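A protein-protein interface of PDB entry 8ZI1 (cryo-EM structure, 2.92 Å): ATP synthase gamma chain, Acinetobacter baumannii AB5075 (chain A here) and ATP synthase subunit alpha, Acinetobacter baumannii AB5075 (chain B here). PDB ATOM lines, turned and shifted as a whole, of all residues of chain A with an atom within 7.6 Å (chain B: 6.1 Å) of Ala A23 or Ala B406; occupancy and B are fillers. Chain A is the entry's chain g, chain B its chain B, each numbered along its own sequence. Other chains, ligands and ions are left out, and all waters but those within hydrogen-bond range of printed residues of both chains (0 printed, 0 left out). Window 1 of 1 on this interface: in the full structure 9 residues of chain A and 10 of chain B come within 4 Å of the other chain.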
ATOM      1  N   SER A  16      -9.170  23.864  13.344  1.00  0.00           N
ATOM      2  CA  SER A  16      -8.235  22.752  13.488  1.00  0.00           C
ATOM      3  C   SER A  16      -7.043  22.903  12.547  1.00  0.00           C
ATOM      4  O   SER A  16      -5.889  22.677  12.944  1.00  0.00           O
ATOM      5  CB  SER A  16      -8.954  21.430  13.234  1.00  0.00           C
ATOM      6  OG  SER A  16      -9.396  21.348  11.892  1.00  0.00           O
ATOM      7  N   THR A  17      -7.303  23.291  11.296  1.00  0.00           N
ATOM      8  CA  THR A  17      -6.206  23.489  10.353  1.00  0.00           C
ATOM      9  C   THR A  17      -5.285  24.614  10.809  1.00  0.00           C
ATOM     10  O   THR A  17      -4.063  24.541  10.628  1.00  0.00           O
ATOM     11  CB  THR A  17      -6.754  23.777   8.956  1.00  0.00           C
ATOM     12  OG1 THR A  17      -7.655  24.888   9.016  1.00  0.00           O
ATOM     13  CG2 THR A  17      -7.490  22.565   8.415  1.00  0.00           C
ATOM     14  N   GLN A  18      -5.853  25.667  11.400  1.00  0.00           N
ATOM     15  CA  GLN A  18      -5.040  26.759  11.921  1.00  0.00           C
ATOM     16  C   GLN A  18      -4.127  26.277  13.038  1.00  0.00           C
ATOM     17  O   GLN A  18      -2.948  26.649  13.093  1.00  0.00           O
ATOM     18  CB  GLN A  18      -5.943  27.888  12.414  1.00  0.00           C
ATOM     19  CG  GLN A  18      -5.208  29.163  12.771  1.00  0.00           C
ATOM     20  CD  GLN A  18      -6.142  30.248  13.257  1.00  0.00           C
ATOM     21  OE1 GLN A  18      -7.239  29.968  13.738  1.00  0.00           O
ATOM     22  NE2 GLN A  18      -5.715  31.498  13.129  1.00  0.00           N
ATOM     23  N   LYS A  19      -4.655  25.449  13.941  1.00  0.00           N
ATOM     24  CA  LYS A  19      -3.816  24.897  15.002  1.00  0.00           C
ATOM     25  C   LYS A  19      -2.675  24.069  14.423  1.00  0.00           C
ATOM     26  O   LYS A  19      -1.521  24.178  14.867  1.00  0.00           O
ATOM     27  CB  LYS A  19      -4.658  24.049  15.953  1.00  0.00           C
ATOM     28  CG  LYS A  19      -5.772  24.808  16.644  1.00  0.00           C
ATOM     29  CD  LYS A  19      -6.563  23.897  17.564  1.00  0.00           C
ATOM     30  CE  LYS A  19      -7.746  24.624  18.173  1.00  0.00           C
ATOM     31  NZ  LYS A  19      -8.532  23.740  19.075  1.00  0.00           N
ATOM     32  N   ILE A  20      -2.978  23.242  13.421  1.00  0.00           N
ATOM     33  CA  ILE A  20      -1.945  22.405  12.813  1.00  0.00           C
ATOM     34  C   ILE A  20      -0.871  23.267  12.156  1.00  0.00           C
ATOM     35  O   ILE A  20       0.333  22.992  12.274  1.00  0.00           O
ATOM     36  CB  ILE A  20      -2.580  21.421  11.816  1.00  0.00           C
ATOM     37  CG1 ILE A  20      -3.343  20.333  12.572  1.00  0.00           C
ATOM     38  CG2 ILE A  20      -1.521  20.802  10.924  1.00  0.00           C
ATOM     39  CD1 ILE A  20      -4.322  19.572  11.721  1.00  0.00           C
ATOM     40  N   THR A  21      -1.285  24.323  11.455  1.00  0.00           N
ATOM     41  CA  THR A  21      -0.319  25.199  10.799  1.00  0.00           C
ATOM     42  C   THR A  21       0.549  25.934  11.816  1.00  0.00           C
ATOM     43  O   THR A  21       1.745  26.142  11.584  1.00  0.00           O
ATOM     44  CB  THR A  21      -1.043  26.189   9.888  1.00  0.00           C
ATOM     45  OG1 THR A  21      -2.142  26.770  10.596  1.00  0.00           O
ATOM     46  CG2 THR A  21      -1.568  25.485   8.650  1.00  0.00           C
ATOM     47  N   ARG A  22      -0.036  26.347  12.945  1.00  0.00           N
ATOM     48  CA  ARG A  22       0.764  26.979  13.994  1.00  0.00           C
ATOM     49  C   ARG A  22       1.805  26.015  14.549  1.00  0.00           C
ATOM     50  O   ARG A  22       2.958  26.401  14.799  1.00  0.00           O
ATOM     51  CB  ARG A  22      -0.141  27.486  15.115  1.00  0.00           C
ATOM     52  CG  ARG A  22      -1.054  28.625  14.710  1.00  0.00           C
ATOM     53  CD  ARG A  22      -2.098  28.899  15.779  1.00  0.00           C
ATOM     54  NE  ARG A  22      -1.523  29.543  16.954  1.00  0.00           N
ATOM     55  CZ  ARG A  22      -1.352  28.950  18.127  1.00  0.00           C
ATOM     56  NH1 ARG A  22      -1.698  27.687  18.318  1.00  0.00           N
ATOM     57  NH2 ARG A  22      -0.821  29.638  19.132  1.00  0.00           N
ATOM     58  N   ALA A  23       1.414  24.756  14.756  1.00  0.00           N
ATOM     59  CA  ALA A  23       2.381  23.759  15.208  1.00  0.00           C
ATOM     60  C   ALA A  23       3.509  23.594  14.198  1.00  0.00           C
ATOM     61  O   ALA A  23       4.687  23.506  14.573  1.00  0.00           O
ATOM     62  CB  ALA A  23       1.683  22.424  15.458  1.00  0.00           C
ATOM     63  N   MET A  24       3.164  23.556  12.907  1.00  0.00           N
ATOM     64  CA  MET A  24       4.188  23.446  11.872  1.00  0.00           C
ATOM     65  C   MET A  24       5.122  24.650  11.889  1.00  0.00           C
ATOM     66  O   MET A  24       6.334  24.507  11.696  1.00  0.00           O
ATOM     67  CB  MET A  24       3.542  23.294  10.496  1.00  0.00           C
ATOM     68  CG  MET A  24       2.902  21.943  10.248  1.00  0.00           C
ATOM     69  SD  MET A  24       2.272  21.785   8.567  1.00  0.00           S
ATOM     70  CE  MET A  24       1.554  20.147   8.627  1.00  0.00           C
ATOM     71  N   GLN A  25       4.573  25.845  12.109  1.00  0.00           N
ATOM     72  CA  GLN A  25       5.405  27.044  12.175  1.00  0.00           C
ATOM     73  C   GLN A  25       6.395  26.970  13.331  1.00  0.00           C
ATOM     74  O   GLN A  25       7.576  27.306  13.171  1.00  0.00           O
ATOM     75  CB  GLN A  25       4.525  28.285  12.309  1.00  0.00           C
ATOM     76  CG  GLN A  25       5.299  29.587  12.321  1.00  0.00           C
ATOM     77  CD  GLN A  25       4.443  30.771  12.710  1.00  0.00           C
ATOM     78  OE1 GLN A  25       3.278  30.617  13.074  1.00  0.00           O
ATOM     79  NE2 GLN A  25       5.016  31.966  12.638  1.00  0.00           N
ATOM     80  N   MET A  26       5.932  26.542  14.506  1.00  0.00           N
ATOM     81  CA  MET A  26       6.836  26.433  15.649  1.00  0.00           C
ATOM     82  C   MET A  26       7.930  25.399  15.396  1.00  0.00           C
ATOM     83  O   MET A  26       9.108  25.630  15.716  1.00  0.00           O
ATOM     84  CB  MET A  26       6.044  26.086  16.907  1.00  0.00           C
ATOM     85  CG  MET A  26       5.123  27.199  17.371  1.00  0.00           C
ATOM     86  SD  MET A  26       4.215  26.785  18.870  1.00  0.00           S
ATOM     87  CE  MET A  26       3.181  28.236  19.048  1.00  0.00           C
ATOM     88  N   VAL A  27       7.559  24.253  14.816  1.00  0.00           N
ATOM     89  CA  VAL A  27       8.549  23.225  14.503  1.00  0.00           C
ATOM     90  C   VAL A  27       9.577  23.762  13.515  1.00  0.00           C
ATOM     91  O   VAL A  27      10.784  23.517  13.651  1.00  0.00           O
ATOM     92  CB  VAL A  27       7.851  21.962  13.966  1.00  0.00           C
ATOM     93  CG1 VAL A  27       8.854  21.038  13.298  1.00  0.00           C
ATOM     94  CG2 VAL A  27       7.126  21.243  15.089  1.00  0.00           C
ATOM     95  N   ALA A  28       9.114  24.501  12.505  1.00  0.00           N
ATOM     96  CA  ALA A  28      10.028  25.076  11.526  1.00  0.00           C
ATOM     97  C   ALA A  28      10.975  26.076  12.173  1.00  0.00           C
ATOM     98  O   ALA A  28      12.156  26.134  11.823  1.00  0.00           O
ATOM     99  CB  ALA A  28       9.240  25.736  10.395  1.00  0.00           C
ATOM    100  N   ALA A  29      10.472  26.878  13.113  1.00  0.00           N
ATOM    101  CA  ALA A  29      11.336  27.827  13.810  1.00  0.00           C
ATOM    102  C   ALA A  29      12.434  27.105  14.580  1.00  0.00           C
ATOM    103  O   ALA A  29      13.610  27.498  14.535  1.00  0.00           O
ATOM    104  CB  ALA A  29      10.504  28.698  14.749  1.00  0.00           C
ATOM    105  N   MET A 249       4.092  29.107   6.290  1.00  0.00           N
ATOM    106  CA  MET A 249       3.149  28.584   7.263  1.00  0.00           C
ATOM    107  C   MET A 249       2.520  29.726   8.039  1.00  0.00           C
ATOM    108  O   MET A 249       1.293  29.789   8.187  1.00  0.00           O
ATOM    109  CB  MET A 249       3.848  27.598   8.198  1.00  0.00           C
ATOM    110  CG  MET A 249       4.423  26.381   7.488  1.00  0.00           C
ATOM    111  SD  MET A 249       3.254  25.509   6.427  1.00  0.00           S
ATOM    112  CE  MET A 249       1.871  25.281   7.538  1.00  0.00           C
ATOM    113  N   THR A 253      -1.596  30.628   8.606  1.00  0.00           N
ATOM    114  CA  THR A 253      -2.294  30.815   9.871  1.00  0.00           C
ATOM    115  C   THR A 253      -3.004  32.156   9.883  1.00  0.00           C
ATOM    116  O   THR A 253      -4.221  32.227  10.099  1.00  0.00           O
ATOM    117  CB  THR A 253      -1.319  30.717  11.044  1.00  0.00           C
ATOM    118  OG1 THR A 253      -0.581  31.940  11.154  1.00  0.00           O
ATOM    119  CG2 THR A 253      -0.354  29.572  10.844  1.00  0.00           C
ATOM    120  N   GLU B 403      -3.435  22.162  25.251  1.00  0.00           N
ATOM    121  CA  GLU B 403      -2.577  23.206  24.699  1.00  0.00           C
ATOM    122  C   GLU B 403      -1.763  22.689  23.520  1.00  0.00           C
ATOM    123  O   GLU B 403      -1.773  23.283  22.436  1.00  0.00           O
ATOM    124  CB  GLU B 403      -1.647  23.743  25.786  1.00  0.00           C
ATOM    125  CG  GLU B 403      -0.762  24.890  25.336  1.00  0.00           C
ATOM    126  CD  GLU B 403       0.110  25.422  26.457  1.00  0.00           C
ATOM    127  OE1 GLU B 403       0.036  24.876  27.578  1.00  0.00           O
ATOM    128  OE2 GLU B 403       0.869  26.384  26.218  1.00  0.00           O
ATOM    129  N   LEU B 404      -1.058  21.578  23.708  1.00  0.00           N
ATOM    130  CA  LEU B 404      -0.168  21.025  22.692  1.00  0.00           C
ATOM    131  C   LEU B 404      -0.617  19.599  22.387  1.00  0.00           C
ATOM    132  O   LEU B 404      -0.421  18.675  23.178  1.00  0.00           O
ATOM    133  CB  LEU B 404       1.314  21.122  23.147  1.00  0.00           C
ATOM    134  CG  LEU B 404       1.914  20.466  24.398  1.00  0.00           C
ATOM    135  CD1 LEU B 404       2.348  19.029  24.171  1.00  0.00           C
ATOM    136  CD2 LEU B 404       3.080  21.292  24.914  1.00  0.00           C
ATOM    137  N   ALA B 405      -1.275  19.434  21.246  1.00  0.00           N
ATOM    138  CA  ALA B 405      -1.702  18.129  20.767  1.00  0.00           C
ATOM    139  C   ALA B 405      -1.359  17.881  19.311  1.00  0.00           C
ATOM    140  O   ALA B 405      -1.160  16.728  18.928  1.00  0.00           O
ATOM    141  CB  ALA B 405      -3.216  17.955  20.957  1.00  0.00           C
ATOM    142  N   ALA B 406      -1.287  18.930  18.491  1.00  0.00           N
ATOM    143  CA  ALA B 406      -0.894  18.780  17.099  1.00  0.00           C
ATOM    144  C   ALA B 406       0.566  18.382  16.945  1.00  0.00           C
ATOM    145  O   ALA B 406       0.967  17.977  15.850  1.00  0.00           O
ATOM    146  CB  ALA B 406      -1.158  20.077  16.336  1.00  0.00           C
ATOM    147  N   PHE B 407       1.360  18.485  18.006  1.00  0.00           N
ATOM    148  CA  PHE B 407       2.763  18.097  17.980  1.00  0.00           C
ATOM    149  C   PHE B 407       2.958  16.591  18.086  1.00  0.00           C
ATOM    150  O   PHE B 407       4.092  16.141  18.279  1.00  0.00           O
ATOM    151  CB  PHE B 407       3.521  18.794  19.113  1.00  0.00           C
ATOM    152  CG  PHE B 407       3.461  20.292  19.054  1.00  0.00           C
ATOM    153  CD1 PHE B 407       2.385  20.977  19.590  1.00  0.00           C
ATOM    154  CD2 PHE B 407       4.484  21.017  18.473  1.00  0.00           C
ATOM    155  CE1 PHE B 407       2.327  22.354  19.540  1.00  0.00           C
ATOM    156  CE2 PHE B 407       4.431  22.395  18.421  1.00  0.00           C
ATOM    157  CZ  PHE B 407       3.351  23.062  18.956  1.00  0.00           C
ATOM    158  N   ALA B 408       1.882  15.809  17.972  1.00  0.00           N
ATOM    159  CA  ALA B 408       1.996  14.361  18.105  1.00  0.00           C
ATOM    160  C   ALA B 408       2.879  13.774  17.012  1.00  0.00           C
ATOM    161  O   ALA B 408       3.696  12.883  17.275  1.00  0.00           O
ATOM    162  CB  ALA B 408       0.609  13.722  18.076  1.00  0.00           C
ATOM    163  N   GLN B 409       2.728  14.257  15.779  1.00  0.00           N
ATOM    164  CA  GLN B 409       3.571  13.773  14.691  1.00  0.00           C
ATOM    165  C   GLN B 409       5.007  14.256  14.850  1.00  0.00           C
ATOM    166  O   GLN B 409       5.952  13.527  14.526  1.00  0.00           O
ATOM    167  CB  GLN B 409       2.998  14.221  13.348  1.00  0.00           C
ATOM    168  CG  GLN B 409       3.904  13.948  12.163  1.00  0.00           C
ATOM    169  CD  GLN B 409       3.467  14.688  10.918  1.00  0.00           C
ATOM    170  OE1 GLN B 409       2.493  15.442  10.939  1.00  0.00           O
ATOM    171  NE2 GLN B 409       4.188  14.481   9.822  1.00  0.00           N
ATOM    172  N   PHE B 410       5.190  15.471  15.359  1.00  0.00           N
ATOM    173  CA  PHE B 410       6.504  16.102  15.459  1.00  0.00           C
ATOM    174  C   PHE B 410       7.090  15.978  16.859  1.00  0.00           C
ATOM    175  O   PHE B 410       7.759  16.894  17.344  1.00  0.00           O
ATOM    176  CB  PHE B 410       6.412  17.567  15.048  1.00  0.00           C
ATOM    177  CG  PHE B 410       5.980  17.771  13.626  1.00  0.00           C
ATOM    178  CD1 PHE B 410       6.867  17.577  12.583  1.00  0.00           C
ATOM    179  CD2 PHE B 410       4.683  18.160  13.334  1.00  0.00           C
ATOM    180  CE1 PHE B 410       6.469  17.766  11.275  1.00  0.00           C
ATOM    181  CE2 PHE B 410       4.280  18.351  12.031  1.00  0.00           C
ATOM    182  CZ  PHE B 410       5.173  18.153  10.999  1.00  0.00           C
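Ala A23 touches Ala B406.
Phe B407 touches Ala A23 (CZ to CB, 3.9 Å).
SD of Met A26 touches CZ of Phe B407, at 3.8 Å.
Phe B410 touches Val A27 (CB to CG2, 3.7 Å).
Of the printed residues of chain B, Ala A23 touches Ala B406 (3.8 Å) and Phe B407 (3.9 Å).
Of chain A, only Ala A23 (3.8 Å) comes within 4 Å of Ala B406.
No residue of chain A comes within 4 Å of Ala B405.
Of the printed residues of chain A, Phe B407 touches Ala A23 and Met A26.
Of the printed residues of chain A, Phe B410 touches Val A27 (3.7 Å).
Thr A17 touches none of the printed residues of chain B.
Met A24 touches none of the printed residues of chain B.
The nearest residue of chain A that does not touch Ala B406 is Ile A20 (4.3 Å).
Of the 8 printed residues of chain B, 3 touch a printed residue of chain A.
Hydrophobic or aromatic side chains of chain B that line the printed part of chain A: Ala B406, Phe B407 and Phe B410.
Hydrophobic or aromatic side chains of chain A within 4 Å of the printed part of chain B: Ala A23, Met A26 and Val A27.
Among the printed residues, no Asp or Glu carboxylate lies within 4 Å of a Lys or Arg side-chain nitrogen of the other chain.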
